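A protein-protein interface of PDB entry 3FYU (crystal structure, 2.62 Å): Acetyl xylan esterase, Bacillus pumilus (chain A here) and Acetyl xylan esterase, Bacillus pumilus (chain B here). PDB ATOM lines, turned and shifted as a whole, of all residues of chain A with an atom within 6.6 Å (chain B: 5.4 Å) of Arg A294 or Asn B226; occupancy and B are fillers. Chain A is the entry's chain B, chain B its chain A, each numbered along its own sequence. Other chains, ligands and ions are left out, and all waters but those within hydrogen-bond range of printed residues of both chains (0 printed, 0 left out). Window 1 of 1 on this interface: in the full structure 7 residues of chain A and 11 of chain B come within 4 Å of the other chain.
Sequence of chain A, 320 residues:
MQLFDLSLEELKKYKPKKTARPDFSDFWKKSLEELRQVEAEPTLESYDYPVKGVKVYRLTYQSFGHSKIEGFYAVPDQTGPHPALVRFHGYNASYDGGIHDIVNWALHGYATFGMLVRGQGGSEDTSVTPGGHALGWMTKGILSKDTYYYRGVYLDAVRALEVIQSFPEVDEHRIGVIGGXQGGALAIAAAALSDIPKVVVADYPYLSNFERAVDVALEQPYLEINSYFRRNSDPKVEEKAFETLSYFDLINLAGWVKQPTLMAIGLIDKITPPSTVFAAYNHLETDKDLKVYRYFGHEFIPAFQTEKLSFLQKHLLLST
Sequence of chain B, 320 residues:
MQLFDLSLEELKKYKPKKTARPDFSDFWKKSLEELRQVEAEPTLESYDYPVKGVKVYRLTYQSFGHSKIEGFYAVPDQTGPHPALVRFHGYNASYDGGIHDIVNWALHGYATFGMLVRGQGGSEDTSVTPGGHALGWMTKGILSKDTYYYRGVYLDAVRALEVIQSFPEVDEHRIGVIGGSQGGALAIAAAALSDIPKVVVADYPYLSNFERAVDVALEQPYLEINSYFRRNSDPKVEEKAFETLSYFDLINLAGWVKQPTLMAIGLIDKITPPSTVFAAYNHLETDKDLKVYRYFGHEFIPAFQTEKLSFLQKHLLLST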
ATOM      1  N   MET A   1      23.262 -12.395 -22.602  1.00  0.00           N
ATOM      2  CA  MET A   1      21.974 -12.189 -21.871  1.00  0.00           C
ATOM      3  C   MET A   1      20.811 -12.075 -22.864  1.00  0.00           C
ATOM      4  O   MET A   1      21.010 -11.851 -24.067  1.00  0.00           O
ATOM      5  CB  MET A   1      22.056 -10.919 -21.012  1.00  0.00           C
ATOM      6  CG  MET A   1      21.532 -11.083 -19.604  1.00  0.00           C
ATOM      7  SD  MET A   1      19.882 -11.812 -19.587  1.00  0.00           S
ATOM      8  CE  MET A   1      20.092 -13.172 -18.366  1.00  0.00           C
ATOM      9  N   GLN A   2      19.597 -12.221 -22.346  1.00  0.00           N
ATOM     10  CA  GLN A   2      18.403 -12.165 -23.179  1.00  0.00           C
ATOM     11  C   GLN A   2      17.334 -11.353 -22.461  1.00  0.00           C
ATOM     12  O   GLN A   2      17.486 -11.044 -21.282  1.00  0.00           O
ATOM     13  CB  GLN A   2      17.906 -13.594 -23.414  1.00  0.00           C
ATOM     14  CG  GLN A   2      16.727 -13.731 -24.372  1.00  0.00           C
ATOM     15  CD  GLN A   2      17.043 -13.195 -25.758  1.00  0.00           C
ATOM     16  OE1 GLN A   2      17.043 -11.985 -25.981  1.00  0.00           O
ATOM     17  NE2 GLN A   2      17.328 -14.097 -26.692  1.00  0.00           N
ATOM     18  N   LEU A   3      16.272 -10.992 -23.180  1.00  0.00           N
ATOM     19  CA  LEU A   3      15.148 -10.259 -22.593  1.00  0.00           C
ATOM     20  C   LEU A   3      14.695 -10.993 -21.322  1.00  0.00           C
ATOM     21  O   LEU A   3      14.805 -12.220 -21.239  1.00  0.00           O
ATOM     22  CB  LEU A   3      13.977 -10.209 -23.577  1.00  0.00           C
ATOM     23  CG  LEU A   3      13.880  -9.118 -24.645  1.00  0.00           C
ATOM     24  CD1 LEU A   3      15.145  -8.267 -24.655  1.00  0.00           C
ATOM     25  CD2 LEU A   3      13.605  -9.762 -25.999  1.00  0.00           C
ATOM     26  N   ILE A 265      18.700   2.991 -21.639  1.00  0.00           N
ATOM     27  CA  ILE A 265      18.461   1.714 -20.988  1.00  0.00           C
ATOM     28  C   ILE A 265      18.637   0.554 -21.961  1.00  0.00           C
ATOM     29  O   ILE A 265      18.178   0.604 -23.100  1.00  0.00           O
ATOM     30  CB  ILE A 265      17.046   1.651 -20.384  1.00  0.00           C
ATOM     31  CG1 ILE A 265      16.843   0.309 -19.674  1.00  0.00           C
ATOM     32  CG2 ILE A 265      16.011   1.864 -21.471  1.00  0.00           C
ATOM     33  CD1 ILE A 265      17.812   0.060 -18.544  1.00  0.00           C
ATOM     34  N   GLY A 266      19.336  -0.479 -21.514  1.00  0.00           N
ATOM     35  CA  GLY A 266      19.510  -1.654 -22.347  1.00  0.00           C
ATOM     36  C   GLY A 266      18.450  -2.625 -21.875  1.00  0.00           C
ATOM     37  O   GLY A 266      18.279  -2.781 -20.670  1.00  0.00           O
ATOM     38  N   LEU A 267      17.733  -3.271 -22.794  1.00  0.00           N
ATOM     39  CA  LEU A 267      16.675  -4.197 -22.394  1.00  0.00           C
ATOM     40  C   LEU A 267      17.145  -5.508 -21.786  1.00  0.00           C
ATOM     41  O   LEU A 267      16.336  -6.254 -21.246  1.00  0.00           O
ATOM     42  CB  LEU A 267      15.735  -4.467 -23.562  1.00  0.00           C
ATOM     43  CG  LEU A 267      14.995  -3.210 -24.030  1.00  0.00           C
ATOM     44  CD1 LEU A 267      14.036  -3.551 -25.153  1.00  0.00           C
ATOM     45  CD2 LEU A 267      14.231  -2.609 -22.854  1.00  0.00           C
ATOM     46  N   ILE A 268      18.438  -5.803 -21.854  1.00  0.00           N
ATOM     47  CA  ILE A 268      18.916  -7.031 -21.241  1.00  0.00           C
ATOM     48  C   ILE A 268      19.804  -6.701 -20.046  1.00  0.00           C
ATOM     49  O   ILE A 268      20.617  -7.524 -19.616  1.00  0.00           O
ATOM     50  CB  ILE A 268      19.706  -7.928 -22.229  1.00  0.00           C
ATOM     51  CG1 ILE A 268      20.901  -7.160 -22.801  1.00  0.00           C
ATOM     52  CG2 ILE A 268      18.786  -8.438 -23.317  1.00  0.00           C
ATOM     53  CD1 ILE A 268      21.807  -7.991 -23.677  1.00  0.00           C
ATOM     54  N   VAL A 292      16.162   3.662 -25.899  1.00  0.00           N
ATOM     55  CA  VAL A 292      16.100   2.240 -25.580  1.00  0.00           C
ATOM     56  C   VAL A 292      16.963   1.436 -26.543  1.00  0.00           C
ATOM     57  O   VAL A 292      16.872   1.602 -27.755  1.00  0.00           O
ATOM     58  CB  VAL A 292      14.638   1.701 -25.650  1.00  0.00           C
ATOM     59  CG1 VAL A 292      14.607   0.208 -25.298  1.00  0.00           C
ATOM     60  CG2 VAL A 292      13.743   2.501 -24.714  1.00  0.00           C
ATOM     61  N   TYR A 293      17.786   0.558 -25.983  1.00  0.00           N
ATOM     62  CA  TYR A 293      18.690  -0.275 -26.757  1.00  0.00           C
ATOM     63  C   TYR A 293      18.421  -1.734 -26.466  1.00  0.00           C
ATOM     64  O   TYR A 293      18.825  -2.260 -25.439  1.00  0.00           O
ATOM     65  CB  TYR A 293      20.122   0.100 -26.406  1.00  0.00           C
ATOM     66  CG  TYR A 293      20.390   1.549 -26.728  1.00  0.00           C
ATOM     67  CD1 TYR A 293      20.620   1.952 -28.040  1.00  0.00           C
ATOM     68  CD2 TYR A 293      20.376   2.524 -25.734  1.00  0.00           C
ATOM     69  CE1 TYR A 293      20.829   3.280 -28.359  1.00  0.00           C
ATOM     70  CE2 TYR A 293      20.588   3.860 -26.047  1.00  0.00           C
ATOM     71  CZ  TYR A 293      20.814   4.228 -27.366  1.00  0.00           C
ATOM     72  OH  TYR A 293      21.030   5.547 -27.695  1.00  0.00           O
ATOM     73  N   ARG A 294      17.727  -2.379 -27.390  1.00  0.00           N
ATOM     74  CA  ARG A 294      17.347  -3.771 -27.256  1.00  0.00           C
ATOM     75  C   ARG A 294      18.458  -4.761 -26.938  1.00  0.00           C
ATOM     76  O   ARG A 294      18.310  -5.625 -26.079  1.00  0.00           O
ATOM     77  CB  ARG A 294      16.635  -4.219 -28.531  1.00  0.00           C
ATOM     78  CG  ARG A 294      16.586  -5.724 -28.733  1.00  0.00           C
ATOM     79  CD  ARG A 294      15.654  -6.402 -27.741  1.00  0.00           C
ATOM     80  NE  ARG A 294      15.631  -7.851 -27.926  1.00  0.00           N
ATOM     81  CZ  ARG A 294      16.602  -8.679 -27.546  1.00  0.00           C
ATOM     82  NH1 ARG A 294      17.687  -8.214 -26.946  1.00  0.00           N
ATOM     83  NH2 ARG A 294      16.494  -9.976 -27.794  1.00  0.00           N
ATOM     84  N   TYR A 295      19.583  -4.627 -27.616  1.00  0.00           N
ATOM     85  CA  TYR A 295      20.671  -5.574 -27.460  1.00  0.00           C
ATOM     86  C   TYR A 295      21.771  -5.253 -26.471  1.00  0.00           C
ATOM     87  O   TYR A 295      22.809  -5.914 -26.472  1.00  0.00           O
ATOM     88  CB  TYR A 295      21.269  -5.831 -28.840  1.00  0.00           C
ATOM     89  CG  TYR A 295      20.210  -6.218 -29.849  1.00  0.00           C
ATOM     90  CD1 TYR A 295      19.661  -7.496 -29.842  1.00  0.00           C
ATOM     91  CD2 TYR A 295      19.730  -5.290 -30.776  1.00  0.00           C
ATOM     92  CE1 TYR A 295      18.659  -7.849 -30.735  1.00  0.00           C
ATOM     93  CE2 TYR A 295      18.728  -5.628 -31.677  1.00  0.00           C
ATOM     94  CZ  TYR A 295      18.191  -6.913 -31.657  1.00  0.00           C
ATOM     95  OH  TYR A 295      17.196  -7.265 -32.555  1.00  0.00           O
ATOM     96  N   PHE A 296      21.567  -4.259 -25.620  1.00  0.00           N
ATOM     97  CA  PHE A 296      22.588  -3.927 -24.647  1.00  0.00           C
ATOM     98  C   PHE A 296      22.141  -4.097 -23.211  1.00  0.00           C
ATOM     99  O   PHE A 296      20.954  -4.160 -22.915  1.00  0.00           O
ATOM    100  CB  PHE A 296      23.084  -2.504 -24.870  1.00  0.00           C
ATOM    101  CG  PHE A 296      23.926  -2.351 -26.099  1.00  0.00           C
ATOM    102  CD1 PHE A 296      23.340  -2.204 -27.344  1.00  0.00           C
ATOM    103  CD2 PHE A 296      25.317  -2.390 -26.013  1.00  0.00           C
ATOM    104  CE1 PHE A 296      24.120  -2.100 -28.484  1.00  0.00           C
ATOM    105  CE2 PHE A 296      26.103  -2.287 -27.149  1.00  0.00           C
ATOM    106  CZ  PHE A 296      25.500  -2.141 -28.390  1.00  0.00           C
ATOM    107  N   GLY A 297      23.115  -4.189 -22.320  1.00  0.00           N
ATOM    108  CA  GLY A 297      22.828  -4.332 -20.906  1.00  0.00           C
ATOM    109  C   GLY A 297      23.457  -3.204 -20.107  1.00  0.00           C
ATOM    110  O   GLY A 297      23.429  -2.041 -20.500  1.00  0.00           O
ATOM    111  N   VAL B 214      15.902 -14.619 -32.180  1.00  0.00           N
ATOM    112  CA  VAL B 214      16.834 -13.709 -31.522  1.00  0.00           C
ATOM    113  C   VAL B 214      16.342 -13.205 -30.188  1.00  0.00           C
ATOM    114  O   VAL B 214      17.113 -12.626 -29.433  1.00  0.00           O
ATOM    115  CB  VAL B 214      17.186 -12.496 -32.399  1.00  0.00           C
ATOM    116  CG1 VAL B 214      17.874 -12.963 -33.667  1.00  0.00           C
ATOM    117  CG2 VAL B 214      15.946 -11.722 -32.727  1.00  0.00           C
ATOM    118  N   ASP B 215      15.065 -13.423 -29.898  1.00  0.00           N
ATOM    119  CA  ASP B 215      14.488 -12.988 -28.624  1.00  0.00           C
ATOM    120  C   ASP B 215      14.235 -14.137 -27.651  1.00  0.00           C
ATOM    121  O   ASP B 215      13.997 -13.905 -26.466  1.00  0.00           O
ATOM    122  CB  ASP B 215      13.175 -12.243 -28.850  1.00  0.00           C
ATOM    123  CG  ASP B 215      13.379 -10.863 -29.442  1.00  0.00           C
ATOM    124  OD1 ASP B 215      14.536 -10.392 -29.510  1.00  0.00           O
ATOM    125  OD2 ASP B 215      12.373 -10.239 -29.831  1.00  0.00           O
ATOM    126  N   TYR B 222      22.126 -18.463 -32.981  1.00  0.00           N
ATOM    127  CA  TYR B 222      21.160 -17.436 -33.345  1.00  0.00           C
ATOM    128  C   TYR B 222      21.628 -16.088 -32.799  1.00  0.00           C
ATOM    129  O   TYR B 222      21.544 -15.057 -33.464  1.00  0.00           O
ATOM    130  CB  TYR B 222      19.785 -17.752 -32.757  1.00  0.00           C
ATOM    131  CG  TYR B 222      18.885 -18.589 -33.636  1.00  0.00           C
ATOM    132  CD1 TYR B 222      18.599 -18.211 -34.949  1.00  0.00           C
ATOM    133  CD2 TYR B 222      18.295 -19.747 -33.142  1.00  0.00           C
ATOM    134  CE1 TYR B 222      17.747 -18.968 -35.746  1.00  0.00           C
ATOM    135  CE2 TYR B 222      17.442 -20.509 -33.926  1.00  0.00           C
ATOM    136  CZ  TYR B 222      17.170 -20.117 -35.222  1.00  0.00           C
ATOM    137  OH  TYR B 222      16.306 -20.877 -35.975  1.00  0.00           O
ATOM    138  N   LEU B 223      22.137 -16.108 -31.579  1.00  0.00           N
ATOM    139  CA  LEU B 223      22.592 -14.891 -30.939  1.00  0.00           C
ATOM    140  C   LEU B 223      23.712 -14.166 -31.694  1.00  0.00           C
ATOM    141  O   LEU B 223      24.057 -13.033 -31.368  1.00  0.00           O
ATOM    142  CB  LEU B 223      23.001 -15.206 -29.502  1.00  0.00           C
ATOM    143  CG  LEU B 223      21.845 -15.866 -28.740  1.00  0.00           C
ATOM    144  CD1 LEU B 223      22.271 -16.204 -27.322  1.00  0.00           C
ATOM    145  CD2 LEU B 223      20.645 -14.926 -28.735  1.00  0.00           C
ATOM    146  N   GLU B 224      24.275 -14.813 -32.703  1.00  0.00           N
ATOM    147  CA  GLU B 224      25.308 -14.170 -33.491  1.00  0.00           C
ATOM    148  C   GLU B 224      24.666 -12.941 -34.110  1.00  0.00           C
ATOM    149  O   GLU B 224      25.317 -11.912 -34.291  1.00  0.00           O
ATOM    150  CB  GLU B 224      25.817 -15.109 -34.595  1.00  0.00           C
ATOM    151  CG  GLU B 224      26.948 -16.021 -34.158  1.00  0.00           C
ATOM    152  CD  GLU B 224      27.430 -16.935 -35.265  1.00  0.00           C
ATOM    153  OE1 GLU B 224      27.418 -16.514 -36.442  1.00  0.00           O
ATOM    154  OE2 GLU B 224      27.842 -18.067 -34.953  1.00  0.00           O
ATOM    155  N   ILE B 225      23.380 -13.058 -34.431  1.00  0.00           N
ATOM    156  CA  ILE B 225      22.638 -11.950 -35.024  1.00  0.00           C
ATOM    157  C   ILE B 225      22.592 -10.804 -34.021  1.00  0.00           C
ATOM    158  O   ILE B 225      22.827  -9.658 -34.384  1.00  0.00           O
ATOM    159  CB  ILE B 225      21.204 -12.380 -35.404  1.00  0.00           C
ATOM    160  CG1 ILE B 225      21.274 -13.468 -36.473  1.00  0.00           C
ATOM    161  CG2 ILE B 225      20.414 -11.196 -35.927  1.00  0.00           C
ATOM    162  CD1 ILE B 225      19.939 -14.073 -36.831  1.00  0.00           C
ATOM    163  N   ASN B 226      22.297 -11.134 -32.764  1.00  0.00           N
ATOM    164  CA  ASN B 226      22.246 -10.156 -31.679  1.00  0.00           C
ATOM    165  C   ASN B 226      23.607  -9.467 -31.562  1.00  0.00           C
ATOM    166  O   ASN B 226      23.696  -8.236 -31.433  1.00  0.00           O
ATOM    167  CB  ASN B 226      21.910 -10.847 -30.350  1.00  0.00           C
ATOM    168  CG  ASN B 226      20.539 -11.525 -30.365  1.00  0.00           C
ATOM    169  OD1 ASN B 226      20.272 -12.411 -31.184  1.00  0.00           O
ATOM    170  ND2 ASN B 226      19.664 -11.109 -29.455  1.00  0.00           N
ATOM    171  N   SER B 227      24.667 -10.267 -31.624  1.00  0.00           N
ATOM    172  CA  SER B 227      26.017  -9.733 -31.534  1.00  0.00           C
ATOM    173  C   SER B 227      26.289  -8.788 -32.690  1.00  0.00           C
ATOM    174  O   SER B 227      26.986  -7.788 -32.539  1.00  0.00           O
ATOM    175  CB  SER B 227      27.039 -10.864 -31.559  1.00  0.00           C
ATOM    176  OG  SER B 227      26.853 -11.746 -30.464  1.00  0.00           O
ATOM    177  N   TYR B 228      25.737  -9.116 -33.851  1.00  0.00           N
ATOM    178  CA  TYR B 228      25.926  -8.297 -35.042  1.00  0.00           C
ATOM    179  C   TYR B 228      25.304  -6.913 -34.831  1.00  0.00           C
ATOM    180  O   TYR B 228      25.942  -5.885 -35.117  1.00  0.00           O
ATOM    181  CB  TYR B 228      25.307  -8.997 -36.261  1.00  0.00           C
ATOM    182  CG  TYR B 228      25.339  -8.181 -37.523  1.00  0.00           C
ATOM    183  CD1 TYR B 228      26.523  -7.994 -38.232  1.00  0.00           C
ATOM    184  CD2 TYR B 228      24.196  -7.548 -37.985  1.00  0.00           C
ATOM    185  CE1 TYR B 228      26.559  -7.186 -39.373  1.00  0.00           C
ATOM    186  CE2 TYR B 228      24.227  -6.743 -39.114  1.00  0.00           C
ATOM    187  CZ  TYR B 228      25.406  -6.566 -39.802  1.00  0.00           C
ATOM    188  OH  TYR B 228      25.408  -5.754 -40.911  1.00  0.00           O
ATOM    189  N   PHE B 229      24.072  -6.879 -34.316  1.00  0.00           N
ATOM    190  CA  PHE B 229      23.409  -5.595 -34.081  1.00  0.00           C
ATOM    191  C   PHE B 229      24.101  -4.779 -32.998  1.00  0.00           C
ATOM    192  O   PHE B 229      24.055  -3.556 -33.030  1.00  0.00           O
ATOM    193  CB  PHE B 229      21.940  -5.791 -33.719  1.00  0.00           C
ATOM    194  CG  PHE B 229      21.147  -6.490 -34.777  1.00  0.00           C
ATOM    195  CD1 PHE B 229      21.372  -6.224 -36.125  1.00  0.00           C
ATOM    196  CD2 PHE B 229      20.143  -7.389 -34.432  1.00  0.00           C
ATOM    197  CE1 PHE B 229      20.604  -6.843 -37.110  1.00  0.00           C
ATOM    198  CE2 PHE B 229      19.372  -8.011 -35.413  1.00  0.00           C
ATOM    199  CZ  PHE B 229      19.602  -7.738 -36.749  1.00  0.00           C
ATOM    200  N   ARG B 230      24.735  -5.450 -32.039  1.00  0.00           N
ATOM    201  CA  ARG B 230      25.454  -4.742 -30.985  1.00  0.00           C
ATOM    202  C   ARG B 230      26.623  -3.979 -31.608  1.00  0.00           C
ATOM    203  O   ARG B 230      27.011  -2.908 -31.133  1.00  0.00           O
ATOM    204  CB  ARG B 230      26.001  -5.722 -29.941  1.00  0.00           C
ATOM    205  CG  ARG B 230      24.958  -6.286 -28.992  1.00  0.00           C
ATOM    206  CD  ARG B 230      25.504  -7.483 -28.219  1.00  0.00           C
ATOM    207  NE  ARG B 230      26.649  -7.128 -27.390  1.00  0.00           N
ATOM    208  CZ  ARG B 230      26.569  -6.388 -26.294  1.00  0.00           C
ATOM    209  NH1 ARG B 230      25.392  -5.928 -25.891  1.00  0.00           N
ATOM    210  NH2 ARG B 230      27.667  -6.096 -25.616  1.00  0.00           N
ATOM    211  N   ARG B 231      27.167  -4.535 -32.688  1.00  0.00           N
ATOM    212  CA  ARG B 231      28.309  -3.944 -33.373  1.00  0.00           C
ATOM    213  C   ARG B 231      27.934  -2.963 -34.470  1.00  0.00           C
ATOM    214  O   ARG B 231      28.784  -2.237 -34.965  1.00  0.00           O
ATOM    215  CB  ARG B 231      29.211  -5.060 -33.920  1.00  0.00           C
ATOM    216  CG  ARG B 231      29.896  -5.858 -32.811  1.00  0.00           C
ATOM    217  CD  ARG B 231      30.539  -7.148 -33.288  1.00  0.00           C
ATOM    218  NE  ARG B 231      31.302  -7.788 -32.215  1.00  0.00           N
ATOM    219  CZ  ARG B 231      30.774  -8.279 -31.093  1.00  0.00           C
ATOM    220  NH1 ARG B 231      29.464  -8.221 -30.881  1.00  0.00           N
ATOM    221  NH2 ARG B 231      31.562  -8.807 -30.164  1.00  0.00           N
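The backbone carbonyl oxygen (O) of Val B214 sits at hydrogen-bond distance from the side-chain amide nitrogen (NE2) of Gln A2 (3.1 Å).
O of Val B214 is in hydrogen-bond range of NH2 of Arg A294.
O of Asp B215 sits close to NE2 of Gln A2, at 3.3 Å.
The side-chain carboxylate (OD1) of Asp B215 is in salt-bridge range of the guanidinium group (NH2) of Arg A294, 2.6 Å away.
The backbone carbonyl oxygen (O) of Tyr A295 lies within hydrogen-bond range of the guanidinium group (NH1) of Arg B230.
The side-chain amide nitrogen (ND2) of Asn B226 is in hydrogen-bond range of the backbone carbonyl oxygen (O) of Val B214 (3.0 Å).
The side-chain hydroxyl (OG) of Ser B227 lies within hydrogen-bond range of the backbone carbonyl oxygen (O) of Leu B223 (3.2 Å).
The guanidinium group (NH2) of Arg A294 is in hydrogen-bond range of the side-chain amide oxygen (OE1) of Gln A2 (2.8 Å).
O of Phe A296 is in hydrogen-bond range of N of Leu A267 (3.3 Å).
The backbone NH (N) of Ile A268 sits close to the backbone carbonyl oxygen (O) of Phe A296 (3.2 Å).
Among the printed residues, merely in contact across the chains: Phe A296 with Arg B230 (3.2 Å), Tyr A295 with Phe B229 (3.4 Å), Leu A3 with Asp B215 (3.6 Å), Tyr A295 with Asn B226 (3.6 Å), Arg A294 with Asn B226 (3.8 Å) and Gln A2 with Leu B223 (3.98 Å).
Printed residues of chain B within 4 Å of Gln A2: Val B214 (3.1 Å), Asp B215 (3.2 Å) and Leu B223 (3.98 Å).
Printed residues of chain B within 4 Å of Leu A3: Asp B215.
Of chain B, only Val B214 (3.2 Å), Asp B215 (2.6 Å) and Asn B226 (3.8 Å) come within 4 Å of Arg A294.
Of the printed residues of chain A, Val B214 touches Gln A2 and Arg A294.
Of the printed residues of chain A, Leu B223 touches Gln A2.
Asn B226 touches two residues of chain A.
The nearest printed residue of chain B that does not touch Arg A294 is Leu B223 (6.5 Å).
The nearest residue of chain A that does not touch Asn B226 is Gln A2 (4.4 Å).
The nearest printed residue of chain A that does not touch Val B214 is Tyr A295 (4.6 Å).
Of the 12 printed residues of chain B, 6 touch a printed residue of chain A.
Hydrophobic or aromatic side chains of chain B that line the printed part of chain A: Leu B223 and Phe B229.
Of the 13 printed residues of chain A, 5 touch a printed residue of chain B.
Hydrophobic or aromatic side chains of chain A within 4 Å of the printed part of chain B: Leu A3, Tyr A295 and Phe A296.
Along chain A the printed residues that touch a printed residue of chain B span positions 2 to 296.
Among the printed residues, Asp or Glu carboxylates within 4 Å of a Lys or Arg side-chain nitrogen of the other chain: Arg A294 with Asp B215.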
